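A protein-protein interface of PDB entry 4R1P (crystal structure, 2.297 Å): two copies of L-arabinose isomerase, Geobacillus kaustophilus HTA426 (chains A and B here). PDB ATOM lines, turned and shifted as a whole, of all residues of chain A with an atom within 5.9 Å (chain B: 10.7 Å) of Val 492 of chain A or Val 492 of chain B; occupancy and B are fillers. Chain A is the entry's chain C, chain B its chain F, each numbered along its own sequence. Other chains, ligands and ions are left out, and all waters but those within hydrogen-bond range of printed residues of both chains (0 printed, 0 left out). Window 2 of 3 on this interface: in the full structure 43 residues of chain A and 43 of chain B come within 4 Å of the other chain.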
ATOM      1  N   LEU A 487      -9.989 -13.539 -25.662  1.00  0.00           N
ATOM      2  CA  LEU A 487     -11.272 -14.003 -25.152  1.00  0.00           C
ATOM      3  C   LEU A 487     -11.088 -15.248 -24.309  1.00  0.00           C
ATOM      4  O   LEU A 487     -11.705 -15.401 -23.246  1.00  0.00           O
ATOM      5  CB  LEU A 487     -12.250 -14.318 -26.288  1.00  0.00           C
ATOM      6  CG  LEU A 487     -12.963 -13.174 -27.001  1.00  0.00           C
ATOM      7  CD1 LEU A 487     -13.979 -13.744 -27.994  1.00  0.00           C
ATOM      8  CD2 LEU A 487     -13.614 -12.197 -26.021  1.00  0.00           C
ATOM      9  N   LYS A 488     -10.251 -16.155 -24.788  1.00  0.00           N
ATOM     10  CA  LYS A 488      -9.977 -17.365 -24.029  1.00  0.00           C
ATOM     11  C   LYS A 488      -9.264 -17.016 -22.727  1.00  0.00           C
ATOM     12  O   LYS A 488      -9.684 -17.416 -21.643  1.00  0.00           O
ATOM     13  CB  LYS A 488      -9.165 -18.360 -24.867  1.00  0.00           C
ATOM     14  CG  LYS A 488      -9.967 -18.942 -26.014  1.00  0.00           C
ATOM     15  CD  LYS A 488      -9.254 -20.083 -26.726  1.00  0.00           C
ATOM     16  CE  LYS A 488     -10.174 -20.708 -27.783  1.00  0.00           C
ATOM     17  NZ  LYS A 488      -9.558 -21.859 -28.512  1.00  0.00           N
ATOM     18  N   TRP A 489      -8.191 -16.244 -22.824  1.00  0.00           N
ATOM     19  CA  TRP A 489      -7.443 -15.909 -21.613  1.00  0.00           C
ATOM     20  C   TRP A 489      -8.261 -15.124 -20.577  1.00  0.00           C
ATOM     21  O   TRP A 489      -8.209 -15.427 -19.405  1.00  0.00           O
ATOM     22  CB  TRP A 489      -6.146 -15.200 -21.982  1.00  0.00           C
ATOM     23  CG  TRP A 489      -5.335 -16.013 -22.931  1.00  0.00           C
ATOM     24  CD1 TRP A 489      -5.319 -17.381 -23.043  1.00  0.00           C
ATOM     25  CD2 TRP A 489      -4.451 -15.521 -23.942  1.00  0.00           C
ATOM     26  NE1 TRP A 489      -4.458 -17.764 -24.045  1.00  0.00           N
ATOM     27  CE2 TRP A 489      -3.914 -16.640 -24.612  1.00  0.00           C
ATOM     28  CE3 TRP A 489      -4.047 -14.245 -24.331  1.00  0.00           C
ATOM     29  CZ2 TRP A 489      -2.987 -16.518 -25.648  1.00  0.00           C
ATOM     30  CZ3 TRP A 489      -3.128 -14.127 -25.367  1.00  0.00           C
ATOM     31  CH2 TRP A 489      -2.611 -15.256 -26.010  1.00  0.00           C
ATOM     32  N   ASN A 490      -9.027 -14.130 -21.022  1.00  0.00           N
ATOM     33  CA  ASN A 490      -9.974 -13.429 -20.145  1.00  0.00           C
ATOM     34  C   ASN A 490     -10.990 -14.346 -19.458  1.00  0.00           C
ATOM     35  O   ASN A 490     -11.278 -14.193 -18.267  1.00  0.00           O
ATOM     36  CB  ASN A 490     -10.746 -12.384 -20.931  1.00  0.00           C
ATOM     37  CG  ASN A 490      -9.949 -11.127 -21.186  1.00  0.00           C
ATOM     38  OD1 ASN A 490      -8.769 -11.028 -20.841  1.00  0.00           O
ATOM     39  ND2 ASN A 490     -10.596 -10.149 -21.810  1.00  0.00           N
ATOM     40  N   GLU A 491     -11.542 -15.294 -20.212  1.00  0.00           N
ATOM     41  CA  GLU A 491     -12.554 -16.202 -19.657  1.00  0.00           C
ATOM     42  C   GLU A 491     -12.046 -16.990 -18.459  1.00  0.00           C
ATOM     43  O   GLU A 491     -12.791 -17.253 -17.526  1.00  0.00           O
ATOM     44  CB  GLU A 491     -13.079 -17.178 -20.720  1.00  0.00           C
ATOM     45  CG  GLU A 491     -14.171 -18.139 -20.214  1.00  0.00           C
ATOM     46  CD  GLU A 491     -15.437 -17.418 -19.752  1.00  0.00           C
ATOM     47  OE1 GLU A 491     -16.165 -16.888 -20.633  1.00  0.00           O
ATOM     48  OE2 GLU A 491     -15.697 -17.389 -18.514  1.00  0.00           O
ATOM     49  N   VAL A 492     -10.780 -17.381 -18.479  1.00  0.00           N
ATOM     50  CA  VAL A 492     -10.282 -18.117 -17.345  1.00  0.00           C
ATOM     51  C   VAL A 492     -10.031 -17.165 -16.179  1.00  0.00           C
ATOM     52  O   VAL A 492     -10.135 -17.550 -15.026  1.00  0.00           O
ATOM     53  CB  VAL A 492      -9.067 -18.969 -17.717  1.00  0.00           C
ATOM     54  CG1 VAL A 492      -9.331 -19.614 -19.046  1.00  0.00           C
ATOM     55  CG2 VAL A 492      -7.837 -18.132 -17.822  1.00  0.00           C
ATOM     56  N   PHE A 493      -9.748 -15.906 -16.474  1.00  0.00           N
ATOM     57  CA  PHE A 493      -9.577 -14.951 -15.393  1.00  0.00           C
ATOM     58  C   PHE A 493     -10.908 -14.569 -14.756  1.00  0.00           C
ATOM     59  O   PHE A 493     -11.051 -14.592 -13.543  1.00  0.00           O
ATOM     60  CB  PHE A 493      -8.833 -13.713 -15.871  1.00  0.00           C
ATOM     61  CG  PHE A 493      -8.811 -12.603 -14.862  1.00  0.00           C
ATOM     62  CD1 PHE A 493      -7.860 -12.590 -13.846  1.00  0.00           C
ATOM     63  CD2 PHE A 493      -9.741 -11.574 -14.928  1.00  0.00           C
ATOM     64  CE1 PHE A 493      -7.838 -11.581 -12.918  1.00  0.00           C
ATOM     65  CE2 PHE A 493      -9.733 -10.557 -13.996  1.00  0.00           C
ATOM     66  CZ  PHE A 493      -8.781 -10.553 -12.990  1.00  0.00           C
ATOM     67  N   TRP A 494     -11.884 -14.225 -15.587  1.00  0.00           N
ATOM     68  CA  TRP A 494     -13.180 -13.773 -15.103  1.00  0.00           C
ATOM     69  C   TRP A 494     -14.053 -14.884 -14.530  1.00  0.00           C
ATOM     70  O   TRP A 494     -15.007 -14.606 -13.806  1.00  0.00           O
ATOM     71  CB  TRP A 494     -13.915 -12.983 -16.187  1.00  0.00           C
ATOM     72  CG  TRP A 494     -13.256 -11.656 -16.425  1.00  0.00           C
ATOM     73  CD1 TRP A 494     -12.466 -11.309 -17.474  1.00  0.00           C
ATOM     74  CD2 TRP A 494     -13.286 -10.522 -15.548  1.00  0.00           C
ATOM     75  NE1 TRP A 494     -12.017 -10.019 -17.322  1.00  0.00           N
ATOM     76  CE2 TRP A 494     -12.503  -9.515 -16.144  1.00  0.00           C
ATOM     77  CE3 TRP A 494     -13.912 -10.259 -14.321  1.00  0.00           C
ATOM     78  CZ2 TRP A 494     -12.326  -8.255 -15.559  1.00  0.00           C
ATOM     79  CZ3 TRP A 494     -13.732  -9.009 -13.732  1.00  0.00           C
ATOM     80  CH2 TRP A 494     -12.952  -8.022 -14.358  1.00  0.00           C
ATOM     81  N   ARG A 495     -13.726 -16.136 -14.834  1.00  0.00           N
ATOM     82  CA  ARG A 495     -14.473 -17.268 -14.272  1.00  0.00           C
ATOM     83  C   ARG A 495     -14.344 -17.286 -12.745  1.00  0.00           C
ATOM     84  O   ARG A 495     -13.246 -17.433 -12.197  1.00  0.00           O
ATOM     85  CB  ARG A 495     -13.998 -18.598 -14.867  1.00  0.00           C
ATOM     86  CG  ARG A 495     -14.834 -19.803 -14.447  1.00  0.00           C
ATOM     87  CD  ARG A 495     -15.952 -20.111 -15.448  1.00  0.00           C
ATOM     88  NE  ARG A 495     -17.158 -20.609 -14.782  1.00  0.00           N
ATOM     89  CZ  ARG A 495     -18.203 -21.148 -15.408  1.00  0.00           C
ATOM     90  NH1 ARG A 495     -19.249 -21.561 -14.701  1.00  0.00           N
ATOM     91  NH2 ARG A 495     -18.203 -21.281 -16.732  1.00  0.00           N
ATOM     92  N   LEU B 397       2.685 -11.284  -2.673  1.00  0.00           N
ATOM     93  CA  LEU B 397       1.268 -11.080  -2.970  1.00  0.00           C
ATOM     94  C   LEU B 397       0.308 -11.816  -2.026  1.00  0.00           C
ATOM     95  O   LEU B 397      -0.900 -11.820  -2.256  1.00  0.00           O
ATOM     96  CB  LEU B 397       0.967 -11.527  -4.407  1.00  0.00           C
ATOM     97  CG  LEU B 397       1.617 -10.708  -5.523  1.00  0.00           C
ATOM     98  CD1 LEU B 397       1.267 -11.319  -6.880  1.00  0.00           C
ATOM     99  CD2 LEU B 397       1.136  -9.269  -5.428  1.00  0.00           C
ATOM    100  N   HIS B 399      -0.111 -15.123  -1.540  1.00  0.00           N
ATOM    101  CA  HIS B 399      -0.064 -16.544  -1.844  1.00  0.00           C
ATOM    102  C   HIS B 399       1.155 -16.913  -2.672  1.00  0.00           C
ATOM    103  O   HIS B 399       1.434 -18.093  -2.882  1.00  0.00           O
ATOM    104  CB  HIS B 399      -1.342 -16.983  -2.560  1.00  0.00           C
ATOM    105  CG  HIS B 399      -1.622 -16.218  -3.815  1.00  0.00           C
ATOM    106  ND1 HIS B 399      -1.894 -14.866  -3.819  1.00  0.00           N
ATOM    107  CD2 HIS B 399      -1.686 -16.616  -5.107  1.00  0.00           C
ATOM    108  CE1 HIS B 399      -2.099 -14.460  -5.061  1.00  0.00           C
ATOM    109  NE2 HIS B 399      -1.973 -15.503  -5.862  1.00  0.00           N
ATOM    110  N   ARG B 400       1.885 -15.908  -3.138  1.00  0.00           N
ATOM    111  CA  ARG B 400       3.036 -16.144  -4.001  1.00  0.00           C
ATOM    112  C   ARG B 400       3.860 -14.879  -4.127  1.00  0.00           C
ATOM    113  O   ARG B 400       3.373 -13.783  -3.830  1.00  0.00           O
ATOM    114  CB  ARG B 400       2.588 -16.608  -5.397  1.00  0.00           C
ATOM    115  CG  ARG B 400       1.754 -15.581  -6.162  1.00  0.00           C
ATOM    116  CD  ARG B 400       1.344 -16.109  -7.551  1.00  0.00           C
ATOM    117  NE  ARG B 400       0.632 -15.112  -8.341  1.00  0.00           N
ATOM    118  CZ  ARG B 400       1.197 -14.276  -9.210  1.00  0.00           C
ATOM    119  NH1 ARG B 400       2.510 -14.306  -9.440  1.00  0.00           N
ATOM    120  NH2 ARG B 400       0.437 -13.413  -9.868  1.00  0.00           N
ATOM    121  N   ARG B 402       6.193 -12.171  -6.507  1.00  0.00           N
ATOM    122  CA  ARG B 402       6.280 -11.614  -7.856  1.00  0.00           C
ATOM    123  C   ARG B 402       7.545 -10.791  -8.001  1.00  0.00           C
ATOM    124  O   ARG B 402       7.806  -9.873  -7.214  1.00  0.00           O
ATOM    125  CB  ARG B 402       5.048 -10.748  -8.195  1.00  0.00           C
ATOM    126  CG  ARG B 402       5.206  -9.867  -9.445  1.00  0.00           C
ATOM    127  CD  ARG B 402       3.998  -8.937  -9.657  1.00  0.00           C
ATOM    128  NE  ARG B 402       2.779  -9.653 -10.034  1.00  0.00           N
ATOM    129  CZ  ARG B 402       1.543  -9.206  -9.806  1.00  0.00           C
ATOM    130  NH1 ARG B 402       1.344  -8.045  -9.186  1.00  0.00           N
ATOM    131  NH2 ARG B 402       0.499  -9.932 -10.185  1.00  0.00           N
ATOM    132  N   GLU B 470       6.604 -15.797 -10.908  1.00  0.00           N
ATOM    133  CA  GLU B 470       6.318 -14.844 -11.961  1.00  0.00           C
ATOM    134  C   GLU B 470       7.348 -13.717 -12.056  1.00  0.00           C
ATOM    135  O   GLU B 470       7.735 -13.117 -11.046  1.00  0.00           O
ATOM    136  CB  GLU B 470       4.936 -14.236 -11.746  1.00  0.00           C
ATOM    137  CG  GLU B 470       4.645 -13.052 -12.636  1.00  0.00           C
ATOM    138  CD  GLU B 470       3.413 -12.295 -12.189  1.00  0.00           C
ATOM    139  OE1 GLU B 470       3.125 -12.322 -10.972  1.00  0.00           O
ATOM    140  OE2 GLU B 470       2.737 -11.684 -13.052  1.00  0.00           O
ATOM    141  N   LYS B 484      -1.414  -4.546 -18.139  1.00  0.00           N
ATOM    142  CA  LYS B 484      -2.513  -4.820 -17.234  1.00  0.00           C
ATOM    143  C   LYS B 484      -3.134  -6.174 -17.558  1.00  0.00           C
ATOM    144  O   LYS B 484      -3.369  -6.987 -16.668  1.00  0.00           O
ATOM    145  CB  LYS B 484      -3.551  -3.700 -17.328  1.00  0.00           C
ATOM    146  CG  LYS B 484      -4.314  -3.441 -16.040  1.00  0.00           C
ATOM    147  CD  LYS B 484      -5.187  -2.212 -16.173  1.00  0.00           C
ATOM    148  CE  LYS B 484      -4.343  -1.004 -16.566  1.00  0.00           C
ATOM    149  NZ  LYS B 484      -5.123   0.276 -16.609  1.00  0.00           N
ATOM    150  N   ASN B 485      -3.380  -6.423 -18.838  1.00  0.00           N
ATOM    151  CA  ASN B 485      -3.900  -7.719 -19.273  1.00  0.00           C
ATOM    152  C   ASN B 485      -3.006  -8.900 -18.879  1.00  0.00           C
ATOM    153  O   ASN B 485      -3.488  -9.915 -18.370  1.00  0.00           O
ATOM    154  CB  ASN B 485      -4.133  -7.726 -20.783  1.00  0.00           C
ATOM    155  CG  ASN B 485      -5.430  -7.034 -21.169  1.00  0.00           C
ATOM    156  OD1 ASN B 485      -6.331  -6.894 -20.346  1.00  0.00           O
ATOM    157  ND2 ASN B 485      -5.535  -6.613 -22.426  1.00  0.00           N
ATOM    158  N   GLU B 486      -1.705  -8.761 -19.104  1.00  0.00           N
ATOM    159  CA  GLU B 486      -0.778  -9.841 -18.775  1.00  0.00           C
ATOM    160  C   GLU B 486      -0.715 -10.159 -17.276  1.00  0.00           C
ATOM    161  O   GLU B 486      -0.604 -11.325 -16.890  1.00  0.00           O
ATOM    162  CB  GLU B 486       0.605  -9.547 -19.335  1.00  0.00           C
ATOM    163  CG  GLU B 486       0.581  -9.285 -20.835  1.00  0.00           C
ATOM    164  CD  GLU B 486       1.953  -8.943 -21.387  1.00  0.00           C
ATOM    165  OE1 GLU B 486       2.020  -8.285 -22.449  1.00  0.00           O
ATOM    166  OE2 GLU B 486       2.960  -9.334 -20.753  1.00  0.00           O
ATOM    167  N   LEU B 487      -0.793  -9.136 -16.431  1.00  0.00           N
ATOM    168  CA  LEU B 487      -0.895  -9.393 -15.004  1.00  0.00           C
ATOM    169  C   LEU B 487      -2.088 -10.300 -14.721  1.00  0.00           C
ATOM    170  O   LEU B 487      -1.982 -11.237 -13.948  1.00  0.00           O
ATOM    171  CB  LEU B 487      -1.013  -8.095 -14.212  1.00  0.00           C
ATOM    172  CG  LEU B 487       0.222  -7.196 -14.151  1.00  0.00           C
ATOM    173  CD1 LEU B 487      -0.167  -5.859 -13.534  1.00  0.00           C
ATOM    174  CD2 LEU B 487       1.364  -7.874 -13.355  1.00  0.00           C
ATOM    175  N   LYS B 488      -3.223 -10.027 -15.350  1.00  0.00           N
ATOM    176  CA  LYS B 488      -4.391 -10.871 -15.151  1.00  0.00           C
ATOM    177  C   LYS B 488      -4.133 -12.312 -15.594  1.00  0.00           C
ATOM    178  O   LYS B 488      -4.376 -13.252 -14.845  1.00  0.00           O
ATOM    179  CB  LYS B 488      -5.604 -10.283 -15.869  1.00  0.00           C
ATOM    180  CG  LYS B 488      -6.137  -8.995 -15.232  1.00  0.00           C
ATOM    181  CD  LYS B 488      -7.262  -8.405 -16.069  1.00  0.00           C
ATOM    182  CE  LYS B 488      -8.211  -7.565 -15.238  1.00  0.00           C
ATOM    183  NZ  LYS B 488      -7.508  -6.442 -14.547  1.00  0.00           N
ATOM    184  N   TRP B 489      -3.616 -12.475 -16.805  1.00  0.00           N
ATOM    185  CA  TRP B 489      -3.367 -13.801 -17.378  1.00  0.00           C
ATOM    186  C   TRP B 489      -2.276 -14.560 -16.618  1.00  0.00           C
ATOM    187  O   TRP B 489      -2.404 -15.755 -16.373  1.00  0.00           O
ATOM    188  CB  TRP B 489      -3.034 -13.676 -18.870  1.00  0.00           C
ATOM    189  CG  TRP B 489      -4.144 -13.002 -19.639  1.00  0.00           C
ATOM    190  CD1 TRP B 489      -5.465 -12.996 -19.317  1.00  0.00           C
ATOM    191  CD2 TRP B 489      -4.018 -12.212 -20.829  1.00  0.00           C
ATOM    192  NE1 TRP B 489      -6.173 -12.277 -20.239  1.00  0.00           N
ATOM    193  CE2 TRP B 489      -5.308 -11.782 -21.178  1.00  0.00           C
ATOM    194  CE3 TRP B 489      -2.940 -11.832 -21.630  1.00  0.00           C
ATOM    195  CZ2 TRP B 489      -5.557 -10.988 -22.304  1.00  0.00           C
ATOM    196  CZ3 TRP B 489      -3.183 -11.045 -22.746  1.00  0.00           C
ATOM    197  CH2 TRP B 489      -4.487 -10.633 -23.075  1.00  0.00           C
ATOM    198  N   ASN B 490      -1.214 -13.860 -16.237  1.00  0.00           N
ATOM    199  CA  ASN B 490      -0.208 -14.447 -15.360  1.00  0.00           C
ATOM    200  C   ASN B 490      -0.813 -14.886 -14.045  1.00  0.00           C
ATOM    201  O   ASN B 490      -0.453 -15.925 -13.504  1.00  0.00           O
ATOM    202  CB  ASN B 490       0.911 -13.452 -15.071  1.00  0.00           C
ATOM    203  CG  ASN B 490       1.869 -13.297 -16.229  1.00  0.00           C
ATOM    204  OD1 ASN B 490       1.716 -13.930 -17.275  1.00  0.00           O
ATOM    205  ND2 ASN B 490       2.862 -12.448 -16.049  1.00  0.00           N
ATOM    206  N   GLU B 491      -1.729 -14.076 -13.533  1.00  0.00           N
ATOM    207  CA  GLU B 491      -2.337 -14.323 -12.241  1.00  0.00           C
ATOM    208  C   GLU B 491      -2.981 -15.696 -12.229  1.00  0.00           C
ATOM    209  O   GLU B 491      -2.794 -16.462 -11.297  1.00  0.00           O
ATOM    210  CB  GLU B 491      -3.383 -13.226 -11.893  1.00  0.00           C
ATOM    211  CG  GLU B 491      -2.816 -11.980 -11.119  1.00  0.00           C
ATOM    212  CD  GLU B 491      -3.815 -10.816 -10.981  1.00  0.00           C
ATOM    213  OE1 GLU B 491      -5.000 -11.071 -10.676  1.00  0.00           O
ATOM    214  OE2 GLU B 491      -3.411  -9.643 -11.173  1.00  0.00           O
ATOM    215  N   VAL B 492      -3.736 -16.020 -13.271  1.00  0.00           N
ATOM    216  CA  VAL B 492      -4.440 -17.285 -13.248  1.00  0.00           C
ATOM    217  C   VAL B 492      -3.451 -18.423 -13.452  1.00  0.00           C
ATOM    218  O   VAL B 492      -3.632 -19.499 -12.886  1.00  0.00           O
ATOM    219  CB  VAL B 492      -5.640 -17.332 -14.245  1.00  0.00           C
ATOM    220  CG1 VAL B 492      -6.426 -16.038 -14.175  1.00  0.00           C
ATOM    221  CG2 VAL B 492      -5.162 -17.544 -15.634  1.00  0.00           C
ATOM    222  N   PHE B 493      -2.386 -18.180 -14.218  1.00  0.00           N
ATOM    223  CA  PHE B 493      -1.335 -19.184 -14.333  1.00  0.00           C
ATOM    224  C   PHE B 493      -0.619 -19.522 -13.017  1.00  0.00           C
ATOM    225  O   PHE B 493      -0.508 -20.687 -12.660  1.00  0.00           O
ATOM    226  CB  PHE B 493      -0.283 -18.843 -15.399  1.00  0.00           C
ATOM    227  CG  PHE B 493       0.798 -19.892 -15.523  1.00  0.00           C
ATOM    228  CD1 PHE B 493       0.565 -21.070 -16.235  1.00  0.00           C
ATOM    229  CD2 PHE B 493       2.025 -19.728 -14.899  1.00  0.00           C
ATOM    230  CE1 PHE B 493       1.548 -22.059 -16.342  1.00  0.00           C
ATOM    231  CE2 PHE B 493       3.007 -20.703 -15.007  1.00  0.00           C
ATOM    232  CZ  PHE B 493       2.762 -21.881 -15.737  1.00  0.00           C
ATOM    233  N   TRP B 494      -0.098 -18.517 -12.327  1.00  0.00           N
ATOM    234  CA  TRP B 494       0.746 -18.766 -11.152  1.00  0.00           C
ATOM    235  C   TRP B 494      -0.037 -19.047  -9.872  1.00  0.00           C
ATOM    236  O   TRP B 494       0.556 -19.433  -8.869  1.00  0.00           O
ATOM    237  CB  TRP B 494       1.700 -17.589 -10.905  1.00  0.00           C
ATOM    238  CG  TRP B 494       2.730 -17.421 -11.956  1.00  0.00           C
ATOM    239  CD1 TRP B 494       2.724 -16.515 -12.980  1.00  0.00           C
ATOM    240  CD2 TRP B 494       3.923 -18.189 -12.104  1.00  0.00           C
ATOM    241  NE1 TRP B 494       3.851 -16.669 -13.752  1.00  0.00           N
ATOM    242  CE2 TRP B 494       4.602 -17.691 -13.235  1.00  0.00           C
ATOM    243  CE3 TRP B 494       4.484 -19.250 -11.388  1.00  0.00           C
ATOM    244  CZ2 TRP B 494       5.815 -18.217 -13.666  1.00  0.00           C
ATOM    245  CZ3 TRP B 494       5.685 -19.773 -11.817  1.00  0.00           C
ATOM    246  CH2 TRP B 494       6.338 -19.258 -12.949  1.00  0.00           C
ATOM    247  N   ARG B 495      -1.352 -18.828  -9.912  1.00  0.00           N
ATOM    248  CA  ARG B 495      -2.251 -19.084  -8.783  1.00  0.00           C
ATOM    249  C   ARG B 495      -2.312 -20.571  -8.506  1.00  0.00           C
ATOM    250  O   ARG B 495      -2.677 -21.354  -9.386  1.00  0.00           O
ATOM    251  CB  ARG B 495      -3.674 -18.599  -9.097  1.00  0.00           C
ATOM    252  CG  ARG B 495      -4.064 -17.244  -8.511  1.00  0.00           C
ATOM    253  CD  ARG B 495      -5.307 -16.673  -9.211  1.00  0.00           C
ATOM    254  NE  ARG B 495      -5.733 -15.379  -8.667  1.00  0.00           N
ATOM    255  CZ  ARG B 495      -6.477 -14.492  -9.330  1.00  0.00           C
ATOM    256  NH1 ARG B 495      -6.817 -13.339  -8.755  1.00  0.00           N
ATOM    257  NH2 ARG B 495      -6.875 -14.746 -10.572  1.00  0.00           N
ATOM    258  N   GLY B 496      -1.962 -20.962  -7.285  1.00  0.00           N
ATOM    259  CA  GLY B 496      -2.098 -22.347  -6.873  1.00  0.00           C
ATOM    260  C   GLY B 496      -3.524 -22.853  -7.026  1.00  0.00           C
ATOM    261  O   GLY B 496      -4.489 -22.158  -6.694  1.00  0.00           O
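NE1 of Trp 489 of chain B sits at hydrogen-bond distance from OD1 of Asn 490 of chain A (2.9 Å).
The side-chain carboxylate (OE1) of Glu 491 of chain B lies within salt-bridge range of the guanidinium group (NH1) of Arg 495 of chain B, 3.5 Å away.
Among the printed residues, pairs that only touch across the chains: Trp 489 of chain A with Trp 489 of chain B (3.4 Å), Val 492 of chain A with Val 492 of chain B (3.5 Å), Phe 493 of chain A with Lys 488 of chain B (3.6 Å), Phe 493 of chain A with Glu 491 of chain B (3.7 Å) and Phe 493 of chain A with Val 492 of chain B (3.5 Å).
Of the printed residues of chain B, Trp 489 of chain A touches Trp 489. Glu 491 of chain A touches none of the printed residues of chain B. Val 492 of chain A touches one residue of chain B. Phe 493 of chain A touches three residues of chain B. Of the printed residues of chain A, Lys 488 of chain B touches Phe 493 (3.6 Å). Printed residues of chain A within 4 Å of Trp 489 of chain B: Trp 489 and Asn 490. Of the printed residues of chain A, Glu 491 of chain B touches Phe 493. Val 492 of chain B touches two residues of chain A. Trp 494 of chain B touches none of the printed residues of chain A. The nearest residue of chain B that does not touch Val 492 of chain A is Trp 489 of chain B (5.9 Å). The nearest residue of chain A that does not touch Val 492 of chain B is Trp 489 of chain A (5.3 Å).
Hydrophobic or aromatic side chains of chain A that line the printed part of chain B: Trp 489, Val 492 and Phe 493. Of the 18 printed residues of chain B, 4 touch a printed residue of chain A. Printed residues of chain B that touch a printed residue of chain A: Lys 488, Trp 489, Glu 491 and Val 492. Among the printed residues, 6 pairs touch across the chains. Among the printed residues, no Asp or Glu carboxylate lies within 4 Å of a Lys or Arg side-chain nitrogen of the other chain.
Asn 490 of chain A touches Trp 489 of chain B, but with the chains exchanged Trp 489 of chain A does not touch Asn 490 of chain B (7.7 Å). Val 492 of chain A touches its own counterpart, Val 492 of chain B. Phe 493 of chain A touches Glu 491 of chain B, but with the chains exchanged Glu 491 of chain A does not touch Phe 493 of chain B (10.6 Å). Phe 493 of chain A touches Val 492 of chain B, but with the chains exchanged Val 492 of chain A does not touch Phe 493 of chain B (6.5 Å). 9 positions are printed for both chains.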
